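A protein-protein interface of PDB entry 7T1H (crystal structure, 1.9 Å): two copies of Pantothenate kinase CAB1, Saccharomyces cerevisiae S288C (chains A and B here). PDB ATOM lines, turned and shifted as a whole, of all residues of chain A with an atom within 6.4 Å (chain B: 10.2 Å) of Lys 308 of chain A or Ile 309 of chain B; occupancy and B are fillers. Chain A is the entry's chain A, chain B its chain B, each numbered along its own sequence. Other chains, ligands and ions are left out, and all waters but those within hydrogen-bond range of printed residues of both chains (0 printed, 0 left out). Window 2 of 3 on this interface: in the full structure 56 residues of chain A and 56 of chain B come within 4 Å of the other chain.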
ATOM      1  N   ALA A 303      -4.740 -31.811 -36.154  1.00  0.00           N
ATOM      2  CA  ALA A 303      -3.901 -32.909 -35.602  1.00  0.00           C
ATOM      3  C   ALA A 303      -3.481 -32.545 -34.172  1.00  0.00           C
ATOM      4  O   ALA A 303      -3.624 -33.380 -33.273  1.00  0.00           O
ATOM      5  CB  ALA A 303      -2.692 -33.140 -36.481  1.00  0.00           C
ATOM      6  N   TYR A 304      -2.982 -31.328 -33.990  1.00  0.00           N
ATOM      7  CA  TYR A 304      -2.565 -30.809 -32.679  1.00  0.00           C
ATOM      8  C   TYR A 304      -3.728 -30.909 -31.685  1.00  0.00           C
ATOM      9  O   TYR A 304      -3.524 -31.480 -30.622  1.00  0.00           O
ATOM     10  CB  TYR A 304      -2.072 -29.363 -32.740  1.00  0.00           C
ATOM     11  CG  TYR A 304      -2.037 -28.795 -31.343  1.00  0.00           C
ATOM     12  CD1 TYR A 304      -1.151 -29.293 -30.406  1.00  0.00           C
ATOM     13  CD2 TYR A 304      -2.995 -27.894 -30.925  1.00  0.00           C
ATOM     14  CE1 TYR A 304      -1.188 -28.849 -29.090  1.00  0.00           C
ATOM     15  CE2 TYR A 304      -3.016 -27.406 -29.631  1.00  0.00           C
ATOM     16  CZ  TYR A 304      -2.117 -27.893 -28.710  1.00  0.00           C
ATOM     17  OH  TYR A 304      -2.171 -27.389 -27.449  1.00  0.00           O
ATOM     18  N   LEU A 305      -4.908 -30.411 -32.066  1.00  0.00           N
ATOM     19  CA  LEU A 305      -6.107 -30.335 -31.206  1.00  0.00           C
ATOM     20  C   LEU A 305      -6.578 -31.740 -30.830  1.00  0.00           C
ATOM     21  O   LEU A 305      -6.829 -31.969 -29.627  1.00  0.00           O
ATOM     22  CB  LEU A 305      -7.196 -29.505 -31.886  1.00  0.00           C
ATOM     23  CG  LEU A 305      -6.906 -28.017 -32.033  1.00  0.00           C
ATOM     24  CD1 LEU A 305      -7.918 -27.366 -32.970  1.00  0.00           C
ATOM     25  CD2 LEU A 305      -6.902 -27.294 -30.699  1.00  0.00           C
ATOM     26  N   GLN A 306      -6.556 -32.692 -31.762  1.00  0.00           N
ATOM     27  CA  GLN A 306      -6.886 -34.108 -31.452  1.00  0.00           C
ATOM     28  C   GLN A 306      -5.829 -34.723 -30.523  1.00  0.00           C
ATOM     29  O   GLN A 306      -6.216 -35.492 -29.612  1.00  0.00           O
ATOM     30  CB  GLN A 306      -7.069 -34.898 -32.747  1.00  0.00           C
ATOM     31  CG  GLN A 306      -8.240 -34.407 -33.571  1.00  0.00           C
ATOM     32  CD  GLN A 306      -9.566 -34.820 -32.966  1.00  0.00           C
ATOM     33  OE1 GLN A 306      -9.701 -34.920 -31.760  1.00  0.00           O
ATOM     34  NE2 GLN A 306     -10.572 -34.976 -33.798  1.00  0.00           N
ATOM     35  N   ALA A 307      -4.547 -34.437 -30.740  1.00  0.00           N
ATOM     36  CA  ALA A 307      -3.433 -34.949 -29.908  1.00  0.00           C
ATOM     37  C   ALA A 307      -3.563 -34.353 -28.497  1.00  0.00           C
ATOM     38  O   ALA A 307      -3.262 -35.094 -27.523  1.00  0.00           O
ATOM     39  CB  ALA A 307      -2.101 -34.597 -30.518  1.00  0.00           C
ATOM     40  N   LYS A 308      -3.988 -33.085 -28.391  1.00  0.00           N
ATOM     41  CA  LYS A 308      -4.187 -32.391 -27.089  1.00  0.00           C
ATOM     42  C   LYS A 308      -5.299 -33.106 -26.308  1.00  0.00           C
ATOM     43  O   LYS A 308      -5.079 -33.489 -25.142  1.00  0.00           O
ATOM     44  CB  LYS A 308      -4.467 -30.904 -27.317  1.00  0.00           C
ATOM     45  CG  LYS A 308      -4.706 -30.082 -26.060  1.00  0.00           C
ATOM     46  CD  LYS A 308      -3.523 -30.070 -25.115  1.00  0.00           C
ATOM     47  CE  LYS A 308      -3.709 -29.114 -23.944  1.00  0.00           C
ATOM     48  NZ  LYS A 308      -2.433 -28.928 -23.220  1.00  0.00           N
ATOM     49  N   ILE A 309      -6.444 -33.317 -26.949  1.00  0.00           N
ATOM     50  CA  ILE A 309      -7.630 -33.969 -26.321  1.00  0.00           C
ATOM     51  C   ILE A 309      -7.241 -35.368 -25.822  1.00  0.00           C
ATOM     52  O   ILE A 309      -7.712 -35.747 -24.763  1.00  0.00           O
ATOM     53  CB  ILE A 309      -8.804 -34.008 -27.320  1.00  0.00           C
ATOM     54  CG1 ILE A 309      -9.330 -32.591 -27.535  1.00  0.00           C
ATOM     55  CG2 ILE A 309      -9.900 -34.981 -26.862  1.00  0.00           C
ATOM     56  CD1 ILE A 309     -10.205 -32.406 -28.765  1.00  0.00           C
ATOM     57  N   ASN A 310      -6.390 -36.093 -26.552  1.00  0.00           N
ATOM     58  CA  ASN A 310      -6.090 -37.524 -26.292  1.00  0.00           C
ATOM     59  C   ASN A 310      -4.757 -37.649 -25.536  1.00  0.00           C
ATOM     60  O   ASN A 310      -4.351 -38.760 -25.303  1.00  0.00           O
ATOM     61  CB  ASN A 310      -6.168 -38.317 -27.603  1.00  0.00           C
ATOM     62  CG  ASN A 310      -7.594 -38.392 -28.118  1.00  0.00           C
ATOM     63  OD1 ASN A 310      -8.435 -39.080 -27.539  1.00  0.00           O
ATOM     64  ND2 ASN A 310      -7.900 -37.671 -29.180  1.00  0.00           N
ATOM     65  N   ASN A 311      -4.126 -36.541 -25.149  1.00  0.00           N
ATOM     66  CA  ASN A 311      -2.777 -36.503 -24.504  1.00  0.00           C
ATOM     67  C   ASN A 311      -1.796 -37.414 -25.256  1.00  0.00           C
ATOM     68  O   ASN A 311      -1.203 -38.310 -24.642  1.00  0.00           O
ATOM     69  CB  ASN A 311      -2.815 -36.892 -23.023  1.00  0.00           C
ATOM     70  CG  ASN A 311      -1.525 -36.571 -22.285  1.00  0.00           C
ATOM     71  OD1 ASN A 311      -0.813 -35.612 -22.598  1.00  0.00           O
ATOM     72  ND2 ASN A 311      -1.192 -37.389 -21.303  1.00  0.00           N
ATOM     73  N   ILE A 312      -1.580 -37.123 -26.526  1.00  0.00           N
ATOM     74  CA  ILE A 312      -0.617 -37.815 -27.416  1.00  0.00           C
ATOM     75  C   ILE A 312       0.484 -36.827 -27.816  1.00  0.00           C
ATOM     76  O   ILE A 312       0.150 -35.712 -28.214  1.00  0.00           O
ATOM     77  CB  ILE A 312      -1.379 -38.358 -28.636  1.00  0.00           C
ATOM     78  CG1 ILE A 312      -2.343 -39.480 -28.229  1.00  0.00           C
ATOM     79  CG2 ILE A 312      -0.417 -38.801 -29.727  1.00  0.00           C
ATOM     80  CD1 ILE A 312      -3.211 -39.949 -29.379  1.00  0.00           C
ATOM     81  N   LYS A 344       4.877 -31.727 -28.561  1.00  0.00           N
ATOM     82  CA  LYS A 344       4.381 -32.737 -29.535  1.00  0.00           C
ATOM     83  C   LYS A 344       5.278 -32.676 -30.766  1.00  0.00           C
ATOM     84  O   LYS A 344       5.896 -31.613 -31.006  1.00  0.00           O
ATOM     85  CB  LYS A 344       2.905 -32.491 -29.849  1.00  0.00           C
ATOM     86  CG  LYS A 344       1.964 -32.642 -28.656  1.00  0.00           C
ATOM     87  CD  LYS A 344       0.506 -32.521 -29.003  1.00  0.00           C
ATOM     88  CE  LYS A 344      -0.341 -32.223 -27.795  1.00  0.00           C
ATOM     89  NZ  LYS A 344      -0.254 -33.311 -26.793  1.00  0.00           N
ATOM     90  N   PRO B 158     -18.601 -20.734 -18.230  1.00  0.00           N
ATOM     91  CA  PRO B 158     -17.679 -20.157 -19.212  1.00  0.00           C
ATOM     92  C   PRO B 158     -18.237 -20.205 -20.652  1.00  0.00           C
ATOM     93  O   PRO B 158     -19.171 -20.935 -20.932  1.00  0.00           O
ATOM     94  CB  PRO B 158     -16.425 -21.033 -19.015  1.00  0.00           C
ATOM     95  CG  PRO B 158     -16.974 -22.401 -18.628  1.00  0.00           C
ATOM     96  CD  PRO B 158     -18.220 -22.101 -17.821  1.00  0.00           C
ATOM     97  N   LEU B 160     -16.962 -19.685 -25.126  1.00  0.00           N
ATOM     98  CA  LEU B 160     -15.961 -19.326 -26.165  1.00  0.00           C
ATOM     99  C   LEU B 160     -16.593 -18.284 -27.055  1.00  0.00           C
ATOM    100  O   LEU B 160     -17.776 -18.479 -27.422  1.00  0.00           O
ATOM    101  CB  LEU B 160     -15.614 -20.496 -27.078  1.00  0.00           C
ATOM    102  CG  LEU B 160     -14.575 -21.495 -26.593  1.00  0.00           C
ATOM    103  CD1 LEU B 160     -14.328 -22.527 -27.686  1.00  0.00           C
ATOM    104  CD2 LEU B 160     -13.284 -20.823 -26.160  1.00  0.00           C
ATOM    105  N   ILE B 170     -10.208 -17.090 -31.509  1.00  0.00           N
ATOM    106  CA  ILE B 170     -11.026 -17.835 -30.527  1.00  0.00           C
ATOM    107  C   ILE B 170     -10.615 -17.397 -29.118  1.00  0.00           C
ATOM    108  O   ILE B 170      -9.438 -17.603 -28.746  1.00  0.00           O
ATOM    109  CB  ILE B 170     -10.927 -19.352 -30.756  1.00  0.00           C
ATOM    110  CG1 ILE B 170     -11.359 -19.742 -32.172  1.00  0.00           C
ATOM    111  CG2 ILE B 170     -11.736 -20.105 -29.698  1.00  0.00           C
ATOM    112  CD1 ILE B 170     -11.143 -21.205 -32.476  1.00  0.00           C
ATOM    113  N   LYS B 172     -11.541 -17.534 -24.837  1.00  0.00           N
ATOM    114  CA  LYS B 172     -12.111 -18.291 -23.710  1.00  0.00           C
ATOM    115  C   LYS B 172     -12.450 -17.258 -22.635  1.00  0.00           C
ATOM    116  O   LYS B 172     -11.579 -16.480 -22.322  1.00  0.00           O
ATOM    117  CB  LYS B 172     -11.076 -19.310 -23.229  1.00  0.00           C
ATOM    118  CG  LYS B 172     -11.478 -20.072 -21.976  1.00  0.00           C
ATOM    119  CD  LYS B 172     -10.462 -21.113 -21.539  1.00  0.00           C
ATOM    120  CE  LYS B 172      -9.186 -20.497 -21.020  1.00  0.00           C
ATOM    121  NZ  LYS B 172      -8.421 -21.453 -20.192  1.00  0.00           N
ATOM    122  N   VAL B 182      -7.236 -18.391 -27.123  1.00  0.00           N
ATOM    123  CA  VAL B 182      -6.782 -19.805 -27.010  1.00  0.00           C
ATOM    124  C   VAL B 182      -6.354 -20.309 -28.379  1.00  0.00           C
ATOM    125  O   VAL B 182      -5.684 -21.333 -28.442  1.00  0.00           O
ATOM    126  CB  VAL B 182      -7.842 -20.739 -26.396  1.00  0.00           C
ATOM    127  CG1 VAL B 182      -8.043 -20.467 -24.916  1.00  0.00           C
ATOM    128  CG2 VAL B 182      -9.145 -20.710 -27.150  1.00  0.00           C
ATOM    129  N   GLY B 183      -6.732 -19.627 -29.445  1.00  0.00           N
ATOM    130  CA  GLY B 183      -6.593 -20.246 -30.757  1.00  0.00           C
ATOM    131  C   GLY B 183      -7.123 -19.344 -31.825  1.00  0.00           C
ATOM    132  O   GLY B 183      -7.559 -18.201 -31.529  1.00  0.00           O
ATOM    133  N   GLN B 301     -15.616 -27.146 -36.497  1.00  0.00           N
ATOM    134  CA  GLN B 301     -14.874 -28.284 -35.919  1.00  0.00           C
ATOM    135  C   GLN B 301     -13.804 -27.736 -34.972  1.00  0.00           C
ATOM    136  O   GLN B 301     -13.654 -28.273 -33.894  1.00  0.00           O
ATOM    137  CB  GLN B 301     -14.253 -29.175 -36.996  1.00  0.00           C
ATOM    138  CG  GLN B 301     -13.347 -30.237 -36.401  1.00  0.00           C
ATOM    139  CD  GLN B 301     -12.824 -31.273 -37.365  1.00  0.00           C
ATOM    140  OE1 GLN B 301     -12.534 -32.403 -36.982  1.00  0.00           O
ATOM    141  NE2 GLN B 301     -12.665 -30.883 -38.609  1.00  0.00           N
ATOM    142  N   ILE B 302     -13.039 -26.728 -35.393  1.00  0.00           N
ATOM    143  CA  ILE B 302     -11.981 -26.139 -34.540  1.00  0.00           C
ATOM    144  C   ILE B 302     -12.632 -25.558 -33.274  1.00  0.00           C
ATOM    145  O   ILE B 302     -12.056 -25.709 -32.192  1.00  0.00           O
ATOM    146  CB  ILE B 302     -11.177 -25.101 -35.329  1.00  0.00           C
ATOM    147  CG1 ILE B 302     -10.287 -25.792 -36.355  1.00  0.00           C
ATOM    148  CG2 ILE B 302     -10.387 -24.191 -34.394  1.00  0.00           C
ATOM    149  CD1 ILE B 302      -9.623 -24.837 -37.311  1.00  0.00           C
ATOM    150  N   ALA B 303     -13.771 -24.885 -33.411  1.00  0.00           N
ATOM    151  CA  ALA B 303     -14.508 -24.288 -32.266  1.00  0.00           C
ATOM    152  C   ALA B 303     -14.937 -25.412 -31.311  1.00  0.00           C
ATOM    153  O   ALA B 303     -14.791 -25.245 -30.066  1.00  0.00           O
ATOM    154  CB  ALA B 303     -15.678 -23.498 -32.754  1.00  0.00           C
ATOM    155  N   TYR B 304     -15.391 -26.534 -31.853  1.00  0.00           N
ATOM    156  CA  TYR B 304     -15.819 -27.706 -31.055  1.00  0.00           C
ATOM    157  C   TYR B 304     -14.607 -28.297 -30.328  1.00  0.00           C
ATOM    158  O   TYR B 304     -14.662 -28.560 -29.130  1.00  0.00           O
ATOM    159  CB  TYR B 304     -16.466 -28.781 -31.913  1.00  0.00           C
ATOM    160  CG  TYR B 304     -16.510 -30.070 -31.167  1.00  0.00           C
ATOM    161  CD1 TYR B 304     -17.453 -30.268 -30.167  1.00  0.00           C
ATOM    162  CD2 TYR B 304     -15.539 -31.040 -31.396  1.00  0.00           C
ATOM    163  CE1 TYR B 304     -17.441 -31.436 -29.422  1.00  0.00           C
ATOM    164  CE2 TYR B 304     -15.524 -32.204 -30.664  1.00  0.00           C
ATOM    165  CZ  TYR B 304     -16.470 -32.393 -29.669  1.00  0.00           C
ATOM    166  OH  TYR B 304     -16.425 -33.550 -28.957  1.00  0.00           O
ATOM    167  N   LEU B 305     -13.482 -28.414 -31.014  1.00  0.00           N
ATOM    168  CA  LEU B 305     -12.290 -29.055 -30.401  1.00  0.00           C
ATOM    169  C   LEU B 305     -11.775 -28.149 -29.264  1.00  0.00           C
ATOM    170  O   LEU B 305     -11.445 -28.713 -28.217  1.00  0.00           O
ATOM    171  CB  LEU B 305     -11.250 -29.338 -31.481  1.00  0.00           C
ATOM    172  CG  LEU B 305     -11.651 -30.413 -32.496  1.00  0.00           C
ATOM    173  CD1 LEU B 305     -10.716 -30.447 -33.663  1.00  0.00           C
ATOM    174  CD2 LEU B 305     -11.730 -31.795 -31.860  1.00  0.00           C
ATOM    175  N   GLN B 306     -11.732 -26.816 -29.455  1.00  0.00           N
ATOM    176  CA  GLN B 306     -11.263 -25.846 -28.429  1.00  0.00           C
ATOM    177  C   GLN B 306     -12.217 -25.909 -27.223  1.00  0.00           C
ATOM    178  O   GLN B 306     -11.729 -25.885 -26.092  1.00  0.00           O
ATOM    179  CB  GLN B 306     -11.166 -24.413 -28.955  1.00  0.00           C
ATOM    180  CG  GLN B 306     -10.029 -24.132 -29.946  1.00  0.00           C
ATOM    181  CD  GLN B 306      -8.660 -24.114 -29.302  1.00  0.00           C
ATOM    182  OE1 GLN B 306      -8.509 -24.476 -28.156  1.00  0.00           O
ATOM    183  NE2 GLN B 306      -7.660 -23.650 -30.025  1.00  0.00           N
ATOM    184  N   ALA B 307     -13.526 -25.964 -27.471  1.00  0.00           N
ATOM    185  CA  ALA B 307     -14.590 -26.114 -26.453  1.00  0.00           C
ATOM    186  C   ALA B 307     -14.382 -27.415 -25.679  1.00  0.00           C
ATOM    187  O   ALA B 307     -14.522 -27.400 -24.434  1.00  0.00           O
ATOM    188  CB  ALA B 307     -15.950 -26.070 -27.107  1.00  0.00           C
ATOM    189  N   LYS B 308     -14.002 -28.487 -26.369  1.00  0.00           N
ATOM    190  CA  LYS B 308     -13.736 -29.803 -25.745  1.00  0.00           C
ATOM    191  C   LYS B 308     -12.520 -29.694 -24.812  1.00  0.00           C
ATOM    192  O   LYS B 308     -12.677 -30.020 -23.635  1.00  0.00           O
ATOM    193  CB  LYS B 308     -13.632 -30.893 -26.818  1.00  0.00           C
ATOM    194  CG  LYS B 308     -13.541 -32.304 -26.275  1.00  0.00           C
ATOM    195  CD  LYS B 308     -14.874 -32.862 -25.842  1.00  0.00           C
ATOM    196  CE  LYS B 308     -14.762 -34.218 -25.174  1.00  0.00           C
ATOM    197  NZ  LYS B 308     -16.090 -34.650 -24.677  1.00  0.00           N
ATOM    198  N   ILE B 309     -11.396 -29.140 -25.278  1.00  0.00           N
ATOM    199  CA  ILE B 309     -10.135 -28.963 -24.498  1.00  0.00           C
ATOM    200  C   ILE B 309     -10.440 -28.107 -23.254  1.00  0.00           C
ATOM    201  O   ILE B 309      -9.919 -28.398 -22.186  1.00  0.00           O
ATOM    202  CB  ILE B 309      -9.056 -28.340 -25.411  1.00  0.00           C
ATOM    203  CG1 ILE B 309      -8.612 -29.338 -26.482  1.00  0.00           C
ATOM    204  CG2 ILE B 309      -7.868 -27.791 -24.627  1.00  0.00           C
ATOM    205  CD1 ILE B 309      -7.789 -28.752 -27.582  1.00  0.00           C
ATOM    206  N   ASN B 310     -11.319 -27.117 -23.377  1.00  0.00           N
ATOM    207  CA  ASN B 310     -11.529 -26.095 -22.330  1.00  0.00           C
ATOM    208  C   ASN B 310     -12.760 -26.421 -21.496  1.00  0.00           C
ATOM    209  O   ASN B 310     -13.079 -25.590 -20.667  1.00  0.00           O
ATOM    210  CB  ASN B 310     -11.631 -24.705 -22.948  1.00  0.00           C
ATOM    211  CG  ASN B 310     -10.274 -24.266 -23.429  1.00  0.00           C
ATOM    212  OD1 ASN B 310      -9.335 -24.220 -22.646  1.00  0.00           O
ATOM    213  ND2 ASN B 310     -10.131 -24.017 -24.713  1.00  0.00           N
ATOM    214  N   ASN B 311     -13.426 -27.547 -21.746  1.00  0.00           N
ATOM    215  CA  ASN B 311     -14.650 -27.978 -21.024  1.00  0.00           C
ATOM    216  C   ASN B 311     -15.690 -26.853 -21.074  1.00  0.00           C
ATOM    217  O   ASN B 311     -16.211 -26.483 -20.010  1.00  0.00           O
ATOM    218  CB  ASN B 311     -14.350 -28.341 -19.564  1.00  0.00           C
ATOM    219  CG  ASN B 311     -13.301 -29.424 -19.436  1.00  0.00           C
ATOM    220  OD1 ASN B 311     -12.296 -29.248 -18.748  1.00  0.00           O
ATOM    221  ND2 ASN B 311     -13.499 -30.531 -20.129  1.00  0.00           N
ATOM    222  N   ILE B 312     -15.996 -26.338 -22.269  1.00  0.00           N
ATOM    223  CA  ILE B 312     -16.966 -25.229 -22.453  1.00  0.00           C
ATOM    224  C   ILE B 312     -18.147 -25.762 -23.257  1.00  0.00           C
ATOM    225  O   ILE B 312     -17.917 -26.545 -24.192  1.00  0.00           O
ATOM    226  CB  ILE B 312     -16.295 -24.005 -23.103  1.00  0.00           C
ATOM    227  CG1 ILE B 312     -15.350 -23.331 -22.116  1.00  0.00           C
ATOM    228  CG2 ILE B 312     -17.330 -23.037 -23.667  1.00  0.00           C
ATOM    229  CD1 ILE B 312     -14.470 -22.266 -22.726  1.00  0.00           C
ATOM    230  N   GLN B 313     -19.355 -25.385 -22.843  1.00  0.00           N
ATOM    231  CA  GLN B 313     -20.633 -25.834 -23.445  1.00  0.00           C
ATOM    232  C   GLN B 313     -21.144 -24.759 -24.409  1.00  0.00           C
ATOM    233  O   GLN B 313     -21.795 -25.137 -25.411  1.00  0.00           O
ATOM    234  CB  GLN B 313     -21.624 -26.156 -22.316  1.00  0.00           C
ATOM    235  CG  GLN B 313     -22.957 -26.705 -22.787  1.00  0.00           C
ATOM    236  CD  GLN B 313     -23.921 -26.909 -21.631  1.00  0.00           C
ATOM    237  OE1 GLN B 313     -23.546 -27.383 -20.560  1.00  0.00           O
ATOM    238  NE2 GLN B 313     -25.178 -26.548 -21.832  1.00  0.00           N
ATOM    239  N   ILE B 315     -20.796 -21.665 -27.079  1.00  0.00           N
ATOM    240  CA  ILE B 315     -19.918 -21.111 -28.155  1.00  0.00           C
ATOM    241  C   ILE B 315     -20.684 -20.000 -28.867  1.00  0.00           C
ATOM    242  O   ILE B 315     -21.662 -20.310 -29.591  1.00  0.00           O
ATOM    243  CB  ILE B 315     -19.471 -22.214 -29.138  1.00  0.00           C
ATOM    244  CG1 ILE B 315     -18.747 -23.359 -28.413  1.00  0.00           C
ATOM    245  CG2 ILE B 315     -18.645 -21.611 -30.275  1.00  0.00           C
ATOM    246  CD1 ILE B 315     -18.761 -24.679 -29.164  1.00  0.00           C
ATOM    247  N   LYS B 344     -23.197 -29.391 -26.641  1.00  0.00           N
ATOM    248  CA  LYS B 344     -22.685 -28.000 -26.725  1.00  0.00           C
ATOM    249  C   LYS B 344     -23.635 -27.262 -27.647  1.00  0.00           C
ATOM    250  O   LYS B 344     -24.270 -27.945 -28.458  1.00  0.00           O
ATOM    251  CB  LYS B 344     -21.248 -27.958 -27.262  1.00  0.00           C
ATOM    252  CG  LYS B 344     -20.223 -28.662 -26.393  1.00  0.00           C
ATOM    253  CD  LYS B 344     -18.791 -28.484 -26.872  1.00  0.00           C
ATOM    254  CE  LYS B 344     -17.816 -29.426 -26.208  1.00  0.00           C
ATOM    255  NZ  LYS B 344     -17.869 -29.300 -24.736  1.00  0.00           N
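Among the printed residues, pairs that only touch across the chains: Leu 305 of chain A with Gln 306 of chain B, Leu 305 of chain A with Ile 309 of chain B, Gln 306 of chain A with Leu 305 of chain B, Lys 308 of chain A with Ile 309 of chain B, Ile 309 of chain A with Leu 305 of chain B and Ile 309 of chain A with Ile 309 of chain B.
Of the 11 printed residues of chain A, 4 touch a printed residue of chain B. Hydrophobic or aromatic side chains of chain A that line the printed part of chain B: Leu 305 and Ile 309. Of the 21 printed residues of chain B, 3 touch a printed residue of chain A. Hydrophobic or aromatic side chains of chain B within 4 Å of the printed part of chain A: Leu 305 and Ile 309. Among the printed residues, no Asp or Glu carboxylate lies within 4 Å of a Lys or Arg side-chain nitrogen of the other chain.
Leu 305 of chain A touches Gln 306 of chain B, and with the chains exchanged Gln 306 of chain A touches Leu 305 of chain B. Leu 305 of chain A touches Ile 309 of chain B, and with the chains exchanged Ile 309 of chain A touches Leu 305 of chain B. Lys 308 of chain A touches Ile 309 of chain B, but with the chains exchanged Ile 309 of chain A does not touch Lys 308 of chain B (4.2 Å). Ile 309 of chain B touches its own counterpart, Ile 309 of chain A. Positions printed for both chains: 303, 304, 305, 306, 307, 308, 309, 310, 311, 312 and 344. Of the 6 pairs that touch across the chains among the printed residues, 5 have their exchanged pair printed and touching as well.
No residue of chain B comes within 4 Å of Tyr 304 of chain A. Of the printed residues of chain B, Leu 305 of chain A touches Gln 306 (3.8 Å) and Ile 309 (3.6 Å). Of the printed residues of chain B, Gln 306 of chain A touches Leu 305 (3.7 Å). No residue of chain B comes within 4 Å of Ala 307 of chain A. Of chain B, only Ile 309 (3.7 Å) comes within 4 Å of Lys 308 of chain A. Of the printed residues of chain A, Leu 305 of chain B touches Gln 306 (3.7 Å) and Ile 309 (3.5 Å). Printed residues of chain A within 4 Å of Gln 306 of chain B: Leu 305 (3.8 Å). The nearest residue of chain A that does not touch Ile 309 of chain B is Tyr 304 of chain A (5.4 Å). The nearest printed residue of chain A that does not touch Leu 305 of chain B is Leu 305 of chain A (4.1 Å).
The backbone carbonyl oxygen (O) of Gln 306 of chain A sits at hydrogen-bond distance from the side-chain amide nitrogen (ND2) of Asn 310 of chain A (2.8 Å). The backbone carbonyl oxygen (O) of Val 182 of chain B is in hydrogen-bond range of the side-chain amide nitrogen (NE2) of Gln 306 of chain B (3.4 Å). The side-chain amide nitrogen (ND2) of Asn 310 of chain B is in hydrogen-bond range of the backbone carbonyl oxygen (O) of Gln 306 of chain B.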
